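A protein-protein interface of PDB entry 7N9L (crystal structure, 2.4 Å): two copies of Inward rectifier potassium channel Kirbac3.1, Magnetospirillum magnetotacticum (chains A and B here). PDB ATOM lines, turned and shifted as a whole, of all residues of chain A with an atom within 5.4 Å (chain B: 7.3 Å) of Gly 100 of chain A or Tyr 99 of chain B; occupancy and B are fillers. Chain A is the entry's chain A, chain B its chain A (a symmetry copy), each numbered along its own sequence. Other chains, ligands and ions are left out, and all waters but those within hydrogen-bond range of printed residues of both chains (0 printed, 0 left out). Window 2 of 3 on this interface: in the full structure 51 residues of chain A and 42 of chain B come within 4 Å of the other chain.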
ATOM      1  N   PHE A  89     -35.788 -27.432  12.276  1.00  0.00           N
ATOM      2  CA  PHE A  89     -34.656 -27.244  11.377  1.00  0.00           C
ATOM      3  C   PHE A  89     -33.398 -27.880  11.952  1.00  0.00           C
ATOM      4  O   PHE A  89     -32.590 -28.453  11.214  1.00  0.00           O
ATOM      5  CB  PHE A  89     -34.421 -25.760  11.109  1.00  0.00           C
ATOM      6  CG  PHE A  89     -33.120 -25.474  10.413  1.00  0.00           C
ATOM      7  CD1 PHE A  89     -32.973 -25.732   9.060  1.00  0.00           C
ATOM      8  CD2 PHE A  89     -32.044 -24.955  11.114  1.00  0.00           C
ATOM      9  CE1 PHE A  89     -31.773 -25.474   8.417  1.00  0.00           C
ATOM     10  CE2 PHE A  89     -30.843 -24.695  10.478  1.00  0.00           C
ATOM     11  CZ  PHE A  89     -30.708 -24.954   9.128  1.00  0.00           C
ATOM     12  N   GLN A  92     -33.790 -31.675  11.225  1.00  0.00           N
ATOM     13  CA  GLN A  92     -33.492 -32.020   9.840  1.00  0.00           C
ATOM     14  C   GLN A  92     -32.022 -31.828   9.500  1.00  0.00           C
ATOM     15  O   GLN A  92     -31.548 -32.390   8.507  1.00  0.00           O
ATOM     16  CB  GLN A  92     -34.347 -31.177   8.893  1.00  0.00           C
ATOM     17  CG  GLN A  92     -35.836 -31.336   9.099  1.00  0.00           C
ATOM     18  CD  GLN A  92     -36.642 -30.265   8.388  1.00  0.00           C
ATOM     19  OE1 GLN A  92     -36.150 -29.603   7.472  1.00  0.00           O
ATOM     20  NE2 GLN A  92     -37.886 -30.085   8.813  1.00  0.00           N
ATOM     21  N   THR A  93     -31.296 -31.036  10.286  1.00  0.00           N
ATOM     22  CA  THR A  93     -29.867 -30.851  10.072  1.00  0.00           C
ATOM     23  C   THR A  93     -29.051 -31.929  10.783  1.00  0.00           C
ATOM     24  O   THR A  93     -28.225 -32.597  10.156  1.00  0.00           O
ATOM     25  CB  THR A  93     -29.442 -29.457  10.544  1.00  0.00           C
ATOM     26  OG1 THR A  93     -30.220 -28.463   9.864  1.00  0.00           O
ATOM     27  CG2 THR A  93     -27.966 -29.219  10.258  1.00  0.00           C
ATOM     28  N   GLY A  98     -32.445 -32.922   5.738  1.00  0.00           N
ATOM     29  CA  GLY A  98     -32.272 -31.809   4.825  1.00  0.00           C
ATOM     30  C   GLY A  98     -33.331 -31.709   3.749  1.00  0.00           C
ATOM     31  O   GLY A  98     -33.005 -31.704   2.557  1.00  0.00           O
ATOM     32  N   TYR A  99     -34.601 -31.620   4.154  1.00  0.00           N
ATOM     33  CA  TYR A  99     -35.686 -31.541   3.182  1.00  0.00           C
ATOM     34  C   TYR A  99     -35.415 -30.461   2.140  1.00  0.00           C
ATOM     35  O   TYR A  99     -35.564 -30.691   0.934  1.00  0.00           O
ATOM     36  CB  TYR A  99     -37.015 -31.273   3.891  1.00  0.00           C
ATOM     37  CG  TYR A  99     -37.586 -32.470   4.621  1.00  0.00           C
ATOM     38  CD1 TYR A  99     -37.895 -33.638   3.940  1.00  0.00           C
ATOM     39  CD2 TYR A  99     -37.830 -32.426   5.989  1.00  0.00           C
ATOM     40  CE1 TYR A  99     -38.421 -34.732   4.595  1.00  0.00           C
ATOM     41  CE2 TYR A  99     -38.359 -33.520   6.656  1.00  0.00           C
ATOM     42  CZ  TYR A  99     -38.653 -34.669   5.950  1.00  0.00           C
ATOM     43  OH  TYR A  99     -39.180 -35.766   6.594  1.00  0.00           O
ATOM     44  N   GLY A 100     -35.012 -29.276   2.590  1.00  0.00           N
ATOM     45  CA  GLY A 100     -34.695 -28.176   1.696  1.00  0.00           C
ATOM     46  C   GLY A 100     -35.606 -26.971   1.815  1.00  0.00           C
ATOM     47  O   GLY A 100     -35.367 -25.970   1.124  1.00  0.00           O
ATOM     48  N   LYS A 101     -36.648 -27.015   2.645  1.00  0.00           N
ATOM     49  CA  LYS A 101     -37.486 -25.841   2.859  1.00  0.00           C
ATOM     50  C   LYS A 101     -36.865 -24.908   3.891  1.00  0.00           C
ATOM     51  O   LYS A 101     -36.720 -23.706   3.646  1.00  0.00           O
ATOM     52  CB  LYS A 101     -38.890 -26.276   3.287  1.00  0.00           C
ATOM     53  CG  LYS A 101     -39.751 -25.162   3.865  1.00  0.00           C
ATOM     54  CD  LYS A 101     -41.204 -25.300   3.430  1.00  0.00           C
ATOM     55  CE  LYS A 101     -42.156 -24.639   4.422  1.00  0.00           C
ATOM     56  NZ  LYS A 101     -42.543 -25.564   5.529  1.00  0.00           N
ATOM     57  N   LEU A 102     -36.491 -25.443   5.051  1.00  0.00           N
ATOM     58  CA  LEU A 102     -35.762 -24.684   6.058  1.00  0.00           C
ATOM     59  C   LEU A 102     -34.271 -24.850   5.790  1.00  0.00           C
ATOM     60  O   LEU A 102     -33.753 -25.972   5.826  1.00  0.00           O
ATOM     61  CB  LEU A 102     -36.118 -25.164   7.462  1.00  0.00           C
ATOM     62  CG  LEU A 102     -37.606 -25.144   7.809  1.00  0.00           C
ATOM     63  CD1 LEU A 102     -37.866 -25.916   9.097  1.00  0.00           C
ATOM     64  CD2 LEU A 102     -38.117 -23.711   7.924  1.00  0.00           C
ATOM     65  N   ILE A 103     -33.587 -23.744   5.510  1.00  0.00           N
ATOM     66  CA  ILE A 103     -32.162 -23.793   5.172  1.00  0.00           C
ATOM     67  C   ILE A 103     -31.454 -22.613   5.806  1.00  0.00           C
ATOM     68  O   ILE A 103     -32.053 -21.561   6.071  1.00  0.00           O
ATOM     69  CB  ILE A 103     -31.936 -23.785   3.648  1.00  0.00           C
ATOM     70  CG1 ILE A 103     -32.682 -22.628   2.983  1.00  0.00           C
ATOM     71  CG2 ILE A 103     -32.408 -25.100   3.039  1.00  0.00           C
ATOM     72  CD1 ILE A 103     -32.569 -22.612   1.463  1.00  0.00           C
ATOM     73  N   PRO A 104     -30.158 -22.767   6.081  1.00  0.00           N
ATOM     74  CA  PRO A 104     -29.434 -21.712   6.802  1.00  0.00           C
ATOM     75  C   PRO A 104     -29.147 -20.499   5.932  1.00  0.00           C
ATOM     76  O   PRO A 104     -28.955 -20.600   4.718  1.00  0.00           O
ATOM     77  CB  PRO A 104     -28.134 -22.406   7.231  1.00  0.00           C
ATOM     78  CG  PRO A 104     -27.924 -23.462   6.195  1.00  0.00           C
ATOM     79  CD  PRO A 104     -29.300 -23.936   5.800  1.00  0.00           C
ATOM     80  N   VAL A 113     -24.509 -25.193  11.385  1.00  0.00           N
ATOM     81  CA  VAL A 113     -24.895 -26.397  10.654  1.00  0.00           C
ATOM     82  C   VAL A 113     -23.696 -27.328  10.514  1.00  0.00           C
ATOM     83  O   VAL A 113     -23.788 -28.533  10.778  1.00  0.00           O
ATOM     84  CB  VAL A 113     -25.494 -26.022   9.285  1.00  0.00           C
ATOM     85  CG1 VAL A 113     -25.497 -27.218   8.341  1.00  0.00           C
ATOM     86  CG2 VAL A 113     -26.914 -25.475   9.456  1.00  0.00           C
ATOM     87  N   PHE B  88     -19.307 -24.860   2.392  1.00  0.00           N
ATOM     88  CA  PHE B  88     -20.569 -25.292   2.985  1.00  0.00           C
ATOM     89  C   PHE B  88     -21.293 -26.280   2.081  1.00  0.00           C
ATOM     90  O   PHE B  88     -22.036 -27.136   2.573  1.00  0.00           O
ATOM     91  CB  PHE B  88     -21.452 -24.082   3.284  1.00  0.00           C
ATOM     92  CG  PHE B  88     -20.960 -23.240   4.436  1.00  0.00           C
ATOM     93  CD1 PHE B  88     -20.524 -23.833   5.612  1.00  0.00           C
ATOM     94  CD2 PHE B  88     -20.923 -21.861   4.338  1.00  0.00           C
ATOM     95  CE1 PHE B  88     -20.069 -23.065   6.666  1.00  0.00           C
ATOM     96  CE2 PHE B  88     -20.468 -21.087   5.391  1.00  0.00           C
ATOM     97  CZ  PHE B  88     -20.038 -21.691   6.556  1.00  0.00           C
ATOM     98  N   GLN B  92     -22.550 -29.994   3.304  1.00  0.00           N
ATOM     99  CA  GLN B  92     -23.863 -30.577   3.058  1.00  0.00           C
ATOM    100  C   GLN B  92     -23.786 -31.830   2.199  1.00  0.00           C
ATOM    101  O   GLN B  92     -24.735 -32.622   2.191  1.00  0.00           O
ATOM    102  CB  GLN B  92     -24.774 -29.553   2.382  1.00  0.00           C
ATOM    103  CG  GLN B  92     -24.974 -28.283   3.178  1.00  0.00           C
ATOM    104  CD  GLN B  92     -25.599 -27.171   2.357  1.00  0.00           C
ATOM    105  OE1 GLN B  92     -26.198 -27.415   1.308  1.00  0.00           O
ATOM    106  NE2 GLN B  92     -25.457 -25.939   2.830  1.00  0.00           N
ATOM    107  N   THR B  93     -22.692 -32.022   1.467  1.00  0.00           N
ATOM    108  CA  THR B  93     -22.507 -33.227   0.670  1.00  0.00           C
ATOM    109  C   THR B  93     -21.881 -34.351   1.492  1.00  0.00           C
ATOM    110  O   THR B  93     -22.424 -35.458   1.546  1.00  0.00           O
ATOM    111  CB  THR B  93     -21.647 -32.917  -0.559  1.00  0.00           C
ATOM    112  OG1 THR B  93     -22.254 -31.860  -1.315  1.00  0.00           O
ATOM    113  CG2 THR B  93     -21.508 -34.148  -1.443  1.00  0.00           C
ATOM    114  N   THR B  96     -24.142 -35.487   3.946  1.00  0.00           N
ATOM    115  CA  THR B  96     -25.336 -35.987   3.268  1.00  0.00           C
ATOM    116  C   THR B  96     -26.601 -35.229   3.660  1.00  0.00           C
ATOM    117  O   THR B  96     -27.711 -35.744   3.486  1.00  0.00           O
ATOM    118  CB  THR B  96     -25.539 -37.492   3.512  1.00  0.00           C
ATOM    119  OG1 THR B  96     -26.026 -37.713   4.841  1.00  0.00           O
ATOM    120  CG2 THR B  96     -24.236 -38.246   3.325  1.00  0.00           C
ATOM    121  N   ILE B  97     -26.462 -34.010   4.185  1.00  0.00           N
ATOM    122  CA  ILE B  97     -27.633 -33.184   4.459  1.00  0.00           C
ATOM    123  C   ILE B  97     -28.392 -32.905   3.168  1.00  0.00           C
ATOM    124  O   ILE B  97     -29.609 -33.120   3.079  1.00  0.00           O
ATOM    125  CB  ILE B  97     -27.221 -31.873   5.148  1.00  0.00           C
ATOM    126  CG1 ILE B  97     -26.550 -32.156   6.487  1.00  0.00           C
ATOM    127  CG2 ILE B  97     -28.441 -30.985   5.349  1.00  0.00           C
ATOM    128  CD1 ILE B  97     -25.804 -30.968   7.052  1.00  0.00           C
ATOM    129  N   GLY B  98     -27.686 -32.396   2.158  1.00  0.00           N
ATOM    130  CA  GLY B  98     -28.257 -32.155   0.848  1.00  0.00           C
ATOM    131  C   GLY B  98     -29.505 -31.301   0.855  1.00  0.00           C
ATOM    132  O   GLY B  98     -30.551 -31.728   0.354  1.00  0.00           O
ATOM    133  N   TYR B  99     -29.409 -30.090   1.410  1.00  0.00           N
ATOM    134  CA  TYR B  99     -30.571 -29.210   1.477  1.00  0.00           C
ATOM    135  C   TYR B  99     -31.248 -29.085   0.117  1.00  0.00           C
ATOM    136  O   TYR B  99     -32.474 -29.200   0.004  1.00  0.00           O
ATOM    137  CB  TYR B  99     -30.162 -27.829   1.995  1.00  0.00           C
ATOM    138  CG  TYR B  99     -29.879 -27.779   3.482  1.00  0.00           C
ATOM    139  CD1 TYR B  99     -30.858 -28.114   4.405  1.00  0.00           C
ATOM    140  CD2 TYR B  99     -28.636 -27.381   3.962  1.00  0.00           C
ATOM    141  CE1 TYR B  99     -30.611 -28.065   5.761  1.00  0.00           C
ATOM    142  CE2 TYR B  99     -28.379 -27.329   5.322  1.00  0.00           C
ATOM    143  CZ  TYR B  99     -29.374 -27.672   6.216  1.00  0.00           C
ATOM    144  OH  TYR B  99     -29.139 -27.625   7.571  1.00  0.00           O
ATOM    145  N   GLY B 100     -30.460 -28.852  -0.930  1.00  0.00           N
ATOM    146  CA  GLY B 100     -30.981 -28.742  -2.281  1.00  0.00           C
ATOM    147  C   GLY B 100     -30.819 -27.378  -2.920  1.00  0.00           C
ATOM    148  O   GLY B 100     -31.189 -27.219  -4.092  1.00  0.00           O
ATOM    149  N   LYS B 101     -30.295 -26.378  -2.211  1.00  0.00           N
ATOM    150  CA  LYS B 101     -30.032 -25.081  -2.823  1.00  0.00           C
ATOM    151  C   LYS B 101     -28.699 -25.087  -3.560  1.00  0.00           C
ATOM    152  O   LYS B 101     -28.626 -24.701  -4.732  1.00  0.00           O
ATOM    153  CB  LYS B 101     -30.064 -23.985  -1.755  1.00  0.00           C
ATOM    154  CG  LYS B 101     -29.477 -22.653  -2.195  1.00  0.00           C
ATOM    155  CD  LYS B 101     -30.268 -21.481  -1.628  1.00  0.00           C
ATOM    156  CE  LYS B 101     -29.413 -20.223  -1.513  1.00  0.00           C
ATOM    157  NZ  LYS B 101     -28.668 -20.169  -0.219  1.00  0.00           N
ATOM    158  N   LEU B 102     -27.634 -25.522  -2.892  1.00  0.00           N
ATOM    159  CA  LEU B 102     -26.336 -25.704  -3.529  1.00  0.00           C
ATOM    160  C   LEU B 102     -26.267 -27.129  -4.065  1.00  0.00           C
ATOM    161  O   LEU B 102     -26.360 -28.090  -3.293  1.00  0.00           O
ATOM    162  CB  LEU B 102     -25.205 -25.440  -2.542  1.00  0.00           C
ATOM    163  CG  LEU B 102     -25.231 -24.074  -1.857  1.00  0.00           C
ATOM    164  CD1 LEU B 102     -24.250 -24.040  -0.691  1.00  0.00           C
ATOM    165  CD2 LEU B 102     -24.925 -22.961  -2.855  1.00  0.00           C
ATOM    166  N   ILE B 103     -26.119 -27.267  -5.380  1.00  0.00           N
ATOM    167  CA  ILE B 103     -26.105 -28.589  -6.012  1.00  0.00           C
ATOM    168  C   ILE B 103     -25.072 -28.607  -7.119  1.00  0.00           C
ATOM    169  O   ILE B 103     -24.730 -27.571  -7.706  1.00  0.00           O
ATOM    170  CB  ILE B 103     -27.489 -28.966  -6.577  1.00  0.00           C
ATOM    171  CG1 ILE B 103     -28.037 -27.863  -7.481  1.00  0.00           C
ATOM    172  CG2 ILE B 103     -28.472 -29.215  -5.439  1.00  0.00           C
ATOM    173  CD1 ILE B 103     -29.441 -28.135  -8.008  1.00  0.00           C
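O of Gly 98 of chain A lies close to O of Gly 98 of chain B (3.3 Å).
OG1 of Thr 93 of chain A is in hydrogen-bond range of OH of Tyr 99 of chain B, 2.7 Å away.
The backbone carbonyl oxygen of Gln 92 of chain A is in hydrogen-bond range of the backbone NH of Gly 98 of chain A, 3.0 Å away.
The backbone carbonyl oxygen (O) of Gln 92 of chain B sits at hydrogen-bond distance from the backbone NH (N) of Ile 97 of chain B, at 3.0 Å.
O of Gln 92 of chain B lies within hydrogen-bond range of N of Gly 98 of chain B (3.0 Å).
The backbone carbonyl oxygen (O) of Phe 89 of chain A sits at hydrogen-bond distance from the side-chain hydroxyl (OG1) of Thr 93 of chain A (2.7 Å).
Among the printed residues, merely in contact across the chains: Phe 89 of chain A with Tyr 99 of chain B (3.5 Å), Gly 98 of chain A with Ile 97 of chain B (3.4 Å), Gly 98 of chain A with Tyr 99 of chain B (3.6 Å), Tyr 99 of chain A with Tyr 99 of chain B (3.6 Å), Gly 100 of chain A with Tyr 99 of chain B (3.0 Å), Leu 102 of chain A with Tyr 99 of chain B (3.8 Å), Ile 103 of chain A with Tyr 99 of chain B (3.7 Å), Pro 104 of chain A with Tyr 99 of chain B (3.5 Å), Val 113 of chain A with Ile 97 of chain B (3.98 Å) and Val 113 of chain A with Tyr 99 of chain B (3.6 Å).
Printed residues of chain B within 4 Å of Phe 89 of chain A: Tyr 99.
Of the printed residues of chain B, Thr 93 of chain A touches Tyr 99 (2.7 Å).
Printed residues of chain B within 4 Å of Gly 98 of chain A: Ile 97 (3.4 Å), Gly 98 (3.3 Å) and Tyr 99 (3.6 Å).
Of chain B, only Tyr 99 comes within 4 Å of Gly 100 of chain A.
Of the printed residues of chain B, Leu 102 of chain A touches Tyr 99 (3.8 Å).
Thr 93 of chain B touches none of the printed residues of chain A.
Leu 102 of chain B touches none of the printed residues of chain A.
The nearest residue of chain B that does not touch Gly 100 of chain A is Gly 100 of chain B (5.0 Å).
Hydrophobic or aromatic side chains of chain A within 4 Å of the printed part of chain B: Phe 89, Ile 103, Pro 104 and Val 113.
Along chain A the printed residues that touch a printed residue of chain B span positions 89 to 113.
Hydrophobic or aromatic side chains of chain B that line the printed part of chain A: Ile 97 and Tyr 99.
Gly 98 of chain B touches its own counterpart, Gly 98 of chain A.
Tyr 99 of chain B touches its own counterpart, Tyr 99 of chain A.
Leu 102 of chain A touches Tyr 99 of chain B, but with the chains exchanged Tyr 99 of chain A does not touch Leu 102 of chain B (10.2 Å).
Ile 103 of chain A touches Tyr 99 of chain B, but with the chains exchanged Tyr 99 of chain A does not touch Ile 103 of chain B (9.6 Å).
Positions printed for both chains: 92, 93, 98, 99, 100, 101, 102 and 103.
Of the 12 pairs that touch across the chains among the printed residues, 2 have their exchanged pair printed and touching as well.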
